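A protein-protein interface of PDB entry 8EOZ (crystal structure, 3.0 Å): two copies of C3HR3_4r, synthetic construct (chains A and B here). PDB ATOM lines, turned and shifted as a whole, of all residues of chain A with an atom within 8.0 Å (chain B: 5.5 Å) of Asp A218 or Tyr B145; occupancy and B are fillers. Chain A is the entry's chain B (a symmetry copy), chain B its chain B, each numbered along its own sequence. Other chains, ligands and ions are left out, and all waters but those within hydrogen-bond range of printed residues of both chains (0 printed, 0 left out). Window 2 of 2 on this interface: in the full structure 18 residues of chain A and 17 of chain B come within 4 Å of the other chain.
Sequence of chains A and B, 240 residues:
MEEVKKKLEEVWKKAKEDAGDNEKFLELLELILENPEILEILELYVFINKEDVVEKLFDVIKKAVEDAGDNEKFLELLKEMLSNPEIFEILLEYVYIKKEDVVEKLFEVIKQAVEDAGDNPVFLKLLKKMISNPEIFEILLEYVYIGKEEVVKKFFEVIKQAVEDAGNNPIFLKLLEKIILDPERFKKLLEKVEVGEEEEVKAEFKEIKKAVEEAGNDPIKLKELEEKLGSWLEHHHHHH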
ATOM      1  N   ILE A 171       9.567 -31.590 -13.309  1.00  0.00           N
ATOM      2  CA  ILE A 171       8.142 -31.360 -13.521  1.00  0.00           C
ATOM      3  C   ILE A 171       7.870 -31.024 -14.983  1.00  0.00           C
ATOM      4  O   ILE A 171       6.960 -31.581 -15.606  1.00  0.00           O
ATOM      5  CB  ILE A 171       7.632 -30.250 -12.585  1.00  0.00           C
ATOM      6  CG1 ILE A 171       8.032 -30.540 -11.135  1.00  0.00           C
ATOM      7  CG2 ILE A 171       6.121 -30.104 -12.708  1.00  0.00           C
ATOM      8  CD1 ILE A 171       7.343 -31.746 -10.533  1.00  0.00           C
ATOM      9  N   VAL A 212       5.422 -23.532 -15.020  1.00  0.00           N
ATOM     10  CA  VAL A 212       5.847 -24.512 -14.022  1.00  0.00           C
ATOM     11  C   VAL A 212       6.611 -23.821 -12.899  1.00  0.00           C
ATOM     12  O   VAL A 212       6.374 -24.080 -11.713  1.00  0.00           O
ATOM     13  CB  VAL A 212       6.689 -25.623 -14.677  1.00  0.00           C
ATOM     14  CG1 VAL A 212       7.272 -26.536 -13.609  1.00  0.00           C
ATOM     15  CG2 VAL A 212       5.849 -26.422 -15.654  1.00  0.00           C
ATOM     16  N   GLU A 214       6.409 -20.676 -12.116  1.00  0.00           N
ATOM     17  CA  GLU A 214       5.532 -19.741 -11.419  1.00  0.00           C
ATOM     18  C   GLU A 214       4.831 -20.425 -10.253  1.00  0.00           C
ATOM     19  O   GLU A 214       4.948 -19.993  -9.100  1.00  0.00           O
ATOM     20  CB  GLU A 214       4.510 -19.145 -12.388  1.00  0.00           C
ATOM     21  CG  GLU A 214       3.592 -18.121 -11.739  1.00  0.00           C
ATOM     22  CD  GLU A 214       2.470 -17.673 -12.652  1.00  0.00           C
ATOM     23  OE1 GLU A 214       2.467 -18.069 -13.836  1.00  0.00           O
ATOM     24  OE2 GLU A 214       1.586 -16.926 -12.180  1.00  0.00           O
ATOM     25  N   ALA A 215       4.094 -21.500 -10.536  1.00  0.00           N
ATOM     26  CA  ALA A 215       3.444 -22.259  -9.472  1.00  0.00           C
ATOM     27  C   ALA A 215       4.481 -22.902  -8.559  1.00  0.00           C
ATOM     28  O   ALA A 215       4.461 -22.710  -7.338  1.00  0.00           O
ATOM     29  CB  ALA A 215       2.517 -23.313 -10.074  1.00  0.00           C
ATOM     30  N   GLY A 216       5.399 -23.669  -9.140  1.00  0.00           N
ATOM     31  CA  GLY A 216       6.522 -24.202  -8.395  1.00  0.00           C
ATOM     32  C   GLY A 216       6.162 -25.235  -7.347  1.00  0.00           C
ATOM     33  O   GLY A 216       5.604 -26.289  -7.666  1.00  0.00           O
ATOM     34  N   ASN A 217       6.471 -24.935  -6.087  1.00  0.00           N
ATOM     35  CA  ASN A 217       6.386 -25.913  -5.010  1.00  0.00           C
ATOM     36  C   ASN A 217       4.972 -26.138  -4.502  1.00  0.00           C
ATOM     37  O   ASN A 217       4.802 -26.584  -3.361  1.00  0.00           O
ATOM     38  CB  ASN A 217       7.294 -25.496  -3.853  1.00  0.00           C
ATOM     39  CG  ASN A 217       8.745 -25.821  -4.118  1.00  0.00           C
ATOM     40  OD1 ASN A 217       9.146 -26.036  -5.264  1.00  0.00           O
ATOM     41  ND2 ASN A 217       9.544 -25.867  -3.058  1.00  0.00           N
ATOM     42  N   ASP A 218       3.958 -25.859  -5.309  1.00  0.00           N
ATOM     43  CA  ASP A 218       2.584 -26.092  -4.889  1.00  0.00           C
ATOM     44  C   ASP A 218       1.971 -27.187  -5.749  1.00  0.00           C
ATOM     45  O   ASP A 218       1.739 -26.970  -6.949  1.00  0.00           O
ATOM     46  CB  ASP A 218       1.762 -24.808  -4.986  1.00  0.00           C
ATOM     47  CG  ASP A 218       0.475 -24.883  -4.191  1.00  0.00           C
ATOM     48  OD1 ASP A 218      -0.302 -25.841  -4.392  1.00  0.00           O
ATOM     49  OD2 ASP A 218       0.245 -23.987  -3.352  1.00  0.00           O
ATOM     50  N   PRO A 219       1.693 -28.367  -5.190  1.00  0.00           N
ATOM     51  CA  PRO A 219       1.128 -29.452  -6.006  1.00  0.00           C
ATOM     52  C   PRO A 219      -0.296 -29.194  -6.466  1.00  0.00           C
ATOM     53  O   PRO A 219      -0.742 -29.833  -7.425  1.00  0.00           O
ATOM     54  CB  PRO A 219       1.198 -30.665  -5.070  1.00  0.00           C
ATOM     55  CG  PRO A 219       1.159 -30.076  -3.698  1.00  0.00           C
ATOM     56  CD  PRO A 219       1.896 -28.770  -3.788  1.00  0.00           C
ATOM     57  N   ILE A 220      -1.027 -28.290  -5.813  1.00  0.00           N
ATOM     58  CA  ILE A 220      -2.366 -27.951  -6.282  1.00  0.00           C
ATOM     59  C   ILE A 220      -2.293 -26.944  -7.422  1.00  0.00           C
ATOM     60  O   ILE A 220      -3.023 -27.057  -8.414  1.00  0.00           O
ATOM     61  CB  ILE A 220      -3.222 -27.432  -5.113  1.00  0.00           C
ATOM     62  CG1 ILE A 220      -3.578 -28.578  -4.164  1.00  0.00           C
ATOM     63  CG2 ILE A 220      -4.485 -26.761  -5.627  1.00  0.00           C
ATOM     64  CD1 ILE A 220      -4.480 -29.621  -4.788  1.00  0.00           C
ATOM     65  N   LYS A 221      -1.406 -25.952  -7.308  1.00  0.00           N
ATOM     66  CA  LYS A 221      -1.234 -24.984  -8.386  1.00  0.00           C
ATOM     67  C   LYS A 221      -0.687 -25.640  -9.650  1.00  0.00           C
ATOM     68  O   LYS A 221      -0.919 -25.139 -10.755  1.00  0.00           O
ATOM     69  CB  LYS A 221      -0.311 -23.851  -7.937  1.00  0.00           C
ATOM     70  CG  LYS A 221      -0.867 -22.979  -6.817  1.00  0.00           C
ATOM     71  CD  LYS A 221       0.129 -21.894  -6.423  1.00  0.00           C
ATOM     72  CE  LYS A 221      -0.404 -21.023  -5.298  1.00  0.00           C
ATOM     73  NZ  LYS A 221      -1.598 -20.239  -5.714  1.00  0.00           N
ATOM     74  N   LEU A 222       0.036 -26.754  -9.509  1.00  0.00           N
ATOM     75  CA  LEU A 222       0.553 -27.454 -10.680  1.00  0.00           C
ATOM     76  C   LEU A 222      -0.491 -28.360 -11.317  1.00  0.00           C
ATOM     77  O   LEU A 222      -0.419 -28.626 -12.522  1.00  0.00           O
ATOM     78  CB  LEU A 222       1.791 -28.271 -10.309  1.00  0.00           C
ATOM     79  CG  LEU A 222       3.101 -27.504 -10.129  1.00  0.00           C
ATOM     80  CD1 LEU A 222       4.240 -28.469  -9.858  1.00  0.00           C
ATOM     81  CD2 LEU A 222       3.399 -26.653 -11.352  1.00  0.00           C
ATOM     82  N   LYS A 223      -1.458 -28.846 -10.535  1.00  0.00           N
ATOM     83  CA  LYS A 223      -2.507 -29.691 -11.098  1.00  0.00           C
ATOM     84  C   LYS A 223      -3.362 -28.919 -12.096  1.00  0.00           C
ATOM     85  O   LYS A 223      -3.788 -29.472 -13.117  1.00  0.00           O
ATOM     86  CB  LYS A 223      -3.377 -30.265  -9.982  1.00  0.00           C
ATOM     87  CG  LYS A 223      -4.496 -31.168 -10.479  1.00  0.00           C
ATOM     88  CD  LYS A 223      -5.428 -31.567  -9.349  1.00  0.00           C
ATOM     89  CE  LYS A 223      -6.180 -30.365  -8.801  1.00  0.00           C
ATOM     90  NZ  LYS A 223      -7.081 -29.768  -9.826  1.00  0.00           N
ATOM     91  N   GLU A 224      -3.629 -27.640 -11.815  1.00  0.00           N
ATOM     92  CA  GLU A 224      -4.374 -26.821 -12.766  1.00  0.00           C
ATOM     93  C   GLU A 224      -3.592 -26.603 -14.054  1.00  0.00           C
ATOM     94  O   GLU A 224      -4.191 -26.534 -15.133  1.00  0.00           O
ATOM     95  CB  GLU A 224      -4.741 -25.474 -12.146  1.00  0.00           C
ATOM     96  CG  GLU A 224      -6.149 -25.410 -11.575  1.00  0.00           C
ATOM     97  CD  GLU A 224      -6.715 -24.000 -11.583  1.00  0.00           C
ATOM     98  OE1 GLU A 224      -6.179 -23.146 -12.320  1.00  0.00           O
ATOM     99  OE2 GLU A 224      -7.697 -23.746 -10.854  1.00  0.00           O
ATOM    100  N   ILE B  97       9.341 -30.952  -5.274  1.00  0.00           N
ATOM    101  CA  ILE B  97       8.440 -29.913  -4.792  1.00  0.00           C
ATOM    102  C   ILE B  97       8.598 -29.669  -3.295  1.00  0.00           C
ATOM    103  O   ILE B  97       8.038 -28.702  -2.765  1.00  0.00           O
ATOM    104  CB  ILE B  97       7.009 -30.327  -5.209  1.00  0.00           C
ATOM    105  CG1 ILE B  97       6.865 -30.272  -6.730  1.00  0.00           C
ATOM    106  CG2 ILE B  97       5.935 -29.447  -4.600  1.00  0.00           C
ATOM    107  CD1 ILE B  97       5.481 -30.632  -7.214  1.00  0.00           C
ATOM    108  N   LYS B  99       7.654 -31.739  -0.819  1.00  0.00           N
ATOM    109  CA  LYS B  99       6.483 -32.233  -0.096  1.00  0.00           C
ATOM    110  C   LYS B  99       6.707 -33.629   0.467  1.00  0.00           C
ATOM    111  O   LYS B  99       5.817 -34.482   0.405  1.00  0.00           O
ATOM    112  CB  LYS B  99       5.255 -32.213  -1.000  1.00  0.00           C
ATOM    113  CG  LYS B  99       4.849 -30.825  -1.454  1.00  0.00           C
ATOM    114  CD  LYS B  99       4.631 -29.903  -0.269  1.00  0.00           C
ATOM    115  CE  LYS B  99       4.308 -28.498  -0.733  1.00  0.00           C
ATOM    116  NZ  LYS B  99       5.382 -27.963  -1.612  1.00  0.00           N
ATOM    117  N   VAL B 102       3.913 -34.426   2.954  1.00  0.00           N
ATOM    118  CA  VAL B 102       2.610 -34.831   2.432  1.00  0.00           C
ATOM    119  C   VAL B 102       2.622 -36.303   2.043  1.00  0.00           C
ATOM    120  O   VAL B 102       1.612 -37.002   2.194  1.00  0.00           O
ATOM    121  CB  VAL B 102       2.210 -33.933   1.245  1.00  0.00           C
ATOM    122  CG1 VAL B 102       0.849 -34.340   0.700  1.00  0.00           C
ATOM    123  CG2 VAL B 102       2.202 -32.472   1.666  1.00  0.00           C
ATOM    124  N   LEU B 140      -5.238 -38.496  -3.673  1.00  0.00           N
ATOM    125  CA  LEU B 140      -5.045 -38.721  -2.245  1.00  0.00           C
ATOM    126  C   LEU B 140      -3.951 -37.820  -1.683  1.00  0.00           C
ATOM    127  O   LEU B 140      -4.068 -37.323  -0.557  1.00  0.00           O
ATOM    128  CB  LEU B 140      -4.720 -40.190  -1.985  1.00  0.00           C
ATOM    129  CG  LEU B 140      -5.836 -41.187  -2.304  1.00  0.00           C
ATOM    130  CD1 LEU B 140      -5.408 -42.607  -1.962  1.00  0.00           C
ATOM    131  CD2 LEU B 140      -7.113 -40.811  -1.566  1.00  0.00           C
ATOM    132  N   LEU B 141      -2.880 -37.598  -2.450  1.00  0.00           N
ATOM    133  CA  LEU B 141      -1.847 -36.660  -2.021  1.00  0.00           C
ATOM    134  C   LEU B 141      -2.379 -35.232  -1.994  1.00  0.00           C
ATOM    135  O   LEU B 141      -2.095 -34.475  -1.060  1.00  0.00           O
ATOM    136  CB  LEU B 141      -0.630 -36.757  -2.940  1.00  0.00           C
ATOM    137  CG  LEU B 141       0.285 -37.974  -2.794  1.00  0.00           C
ATOM    138  CD1 LEU B 141       1.352 -37.971  -3.876  1.00  0.00           C
ATOM    139  CD2 LEU B 141       0.925 -37.991  -1.417  1.00  0.00           C
ATOM    140  N   GLU B 142      -3.156 -34.852  -3.012  1.00  0.00           N
ATOM    141  CA  GLU B 142      -3.681 -33.495  -3.102  1.00  0.00           C
ATOM    142  C   GLU B 142      -4.709 -33.192  -2.019  1.00  0.00           C
ATOM    143  O   GLU B 142      -4.918 -32.019  -1.696  1.00  0.00           O
ATOM    144  CB  GLU B 142      -4.283 -33.266  -4.489  1.00  0.00           C
ATOM    145  CG  GLU B 142      -3.243 -33.177  -5.597  1.00  0.00           C
ATOM    146  CD  GLU B 142      -3.816 -33.465  -6.971  1.00  0.00           C
ATOM    147  OE1 GLU B 142      -5.022 -33.775  -7.064  1.00  0.00           O
ATOM    148  OE2 GLU B 142      -3.057 -33.386  -7.961  1.00  0.00           O
ATOM    149  N   TYR B 143      -5.352 -34.213  -1.455  1.00  0.00           N
ATOM    150  CA  TYR B 143      -6.270 -33.997  -0.344  1.00  0.00           C
ATOM    151  C   TYR B 143      -5.551 -33.870   0.989  1.00  0.00           C
ATOM    152  O   TYR B 143      -6.104 -33.279   1.923  1.00  0.00           O
ATOM    153  CB  TYR B 143      -7.290 -35.135  -0.269  1.00  0.00           C
ATOM    154  CG  TYR B 143      -8.636 -34.784  -0.860  1.00  0.00           C
ATOM    155  CD1 TYR B 143      -8.843 -34.813  -2.231  1.00  0.00           C
ATOM    156  CD2 TYR B 143      -9.699 -34.425  -0.044  1.00  0.00           C
ATOM    157  CE1 TYR B 143     -10.071 -34.493  -2.774  1.00  0.00           C
ATOM    158  CE2 TYR B 143     -10.931 -34.105  -0.576  1.00  0.00           C
ATOM    159  CZ  TYR B 143     -11.112 -34.139  -1.941  1.00  0.00           C
ATOM    160  OH  TYR B 143     -12.339 -33.820  -2.475  1.00  0.00           O
ATOM    161  N   VAL B 144      -4.339 -34.405   1.098  1.00  0.00           N
ATOM    162  CA  VAL B 144      -3.579 -34.330   2.342  1.00  0.00           C
ATOM    163  C   VAL B 144      -2.782 -33.034   2.433  1.00  0.00           C
ATOM    164  O   VAL B 144      -2.637 -32.465   3.518  1.00  0.00           O
ATOM    165  CB  VAL B 144      -2.672 -35.571   2.463  1.00  0.00           C
ATOM    166  CG1 VAL B 144      -1.719 -35.430   3.633  1.00  0.00           C
ATOM    167  CG2 VAL B 144      -3.517 -36.828   2.614  1.00  0.00           C
ATOM    168  N   TYR B 145      -2.262 -32.542   1.302  1.00  0.00           N
ATOM    169  CA  TYR B 145      -1.505 -31.293   1.313  1.00  0.00           C
ATOM    170  C   TYR B 145      -2.371 -30.124   1.767  1.00  0.00           C
ATOM    171  O   TYR B 145      -1.895 -29.229   2.476  1.00  0.00           O
ATOM    172  CB  TYR B 145      -0.918 -31.024  -0.072  1.00  0.00           C
ATOM    173  CG  TYR B 145      -0.468 -29.596  -0.293  1.00  0.00           C
ATOM    174  CD1 TYR B 145       0.601 -29.065   0.417  1.00  0.00           C
ATOM    175  CD2 TYR B 145      -1.105 -28.782  -1.223  1.00  0.00           C
ATOM    176  CE1 TYR B 145       1.016 -27.762   0.215  1.00  0.00           C
ATOM    177  CE2 TYR B 145      -0.696 -27.479  -1.435  1.00  0.00           C
ATOM    178  CZ  TYR B 145       0.365 -26.974  -0.713  1.00  0.00           C
ATOM    179  OH  TYR B 145       0.776 -25.676  -0.919  1.00  0.00           O
ATOM    180  N   ILE B 146      -3.646 -30.117   1.372  1.00  0.00           N
ATOM    181  CA  ILE B 146      -4.570 -29.088   1.841  1.00  0.00           C
ATOM    182  C   ILE B 146      -4.774 -29.197   3.346  1.00  0.00           C
ATOM    183  O   ILE B 146      -4.955 -28.184   4.034  1.00  0.00           O
ATOM    184  CB  ILE B 146      -5.907 -29.193   1.078  1.00  0.00           C
ATOM    185  CG1 ILE B 146      -5.676 -29.027  -0.424  1.00  0.00           C
ATOM    186  CG2 ILE B 146      -6.908 -28.163   1.587  1.00  0.00           C
ATOM    187  CD1 ILE B 146      -6.934 -29.160  -1.253  1.00  0.00           C
ATOM    188  N   GLY B 147      -4.730 -30.413   3.882  1.00  0.00           N
ATOM    189  CA  GLY B 147      -4.998 -30.675   5.283  1.00  0.00           C
ATOM    190  C   GLY B 147      -6.167 -31.603   5.519  1.00  0.00           C
ATOM    191  O   GLY B 147      -6.268 -32.196   6.604  1.00  0.00           O
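O of Ile B97 sits at hydrogen-bond distance from ND2 of Asn A217, at 3.2 Å. The side-chain carboxylate of Asp A218 lies within hydrogen-bond range of the side-chain hydroxyl of Tyr B145 (3.0 Å). O of Asn A217 sits close to NZ of Lys B99 (2.3 Å).
O of Ile B97 is in hydrogen-bond range of NZ of Lys B99. The side-chain carboxylate (OD1) of Asp A218 lies within hydrogen-bond range of the backbone NH (N) of Ile A220, 2.9 Å away. N of Lys A221 is in hydrogen-bond range of OD1 of Asp A218, 3.1 Å away.
Among the printed residues, pairs that only touch across the chains: Lys A223 with Glu B142, Pro A219 with Tyr B145, Leu A222 with Ile B97, Ile A220 with Glu B142, Ile A220 with Tyr B145, Pro A219 with Lys B99 and Ile A171 with Ile B97.
Asp A218 touches just one residue of chain B: Tyr B145. Of chain A, only Asp A218, Pro A219 and Ile A220 come within 4 Å of Tyr B145. Of the printed residues of chain B, Leu A222 touches Ile B97 (3.6 Å). Of the printed residues of chain A, Glu B142 touches Ile A220 (3.7 Å) and Lys A223 (3.2 Å). Printed residues of chain A within 4 Å of Ile B97: Ile A171 (3.97 Å), Asn A217 (3.2 Å) and Leu A222 (3.6 Å). Printed residues of chain A within 4 Å of Lys B99: Asn A217 (2.3 Å) and Pro A219 (3.9 Å). Of the printed residues of chain B, Pro A219 touches Lys B99 (3.9 Å) and Tyr B145 (3.6 Å). Val B144 touches none of the printed residues of chain A. The nearest residue of chain B that does not touch Asp A218 is Ile B97 (4.2 Å). The nearest residue of chain A that does not touch Tyr B145 is Asn A217 (4.8 Å).
Of the 11 printed residues of chain B, 4 touch a printed residue of chain A. Hydrophobic or aromatic side chains of chain A within 4 Å of the printed part of chain B: Ile A171, Pro A219, Ile A220 and Leu A222. Along chain A the printed residues that touch a printed residue of chain B span positions 171 to 223. Among the printed residues, no Asp or Glu carboxylate lies within 4 Å of a Lys or Arg side-chain nitrogen of the other chain.
No position is printed for both chains. Of the 10 pairs that touch across the chains among the printed residues, none has its exchanged pair printed and touching as well.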
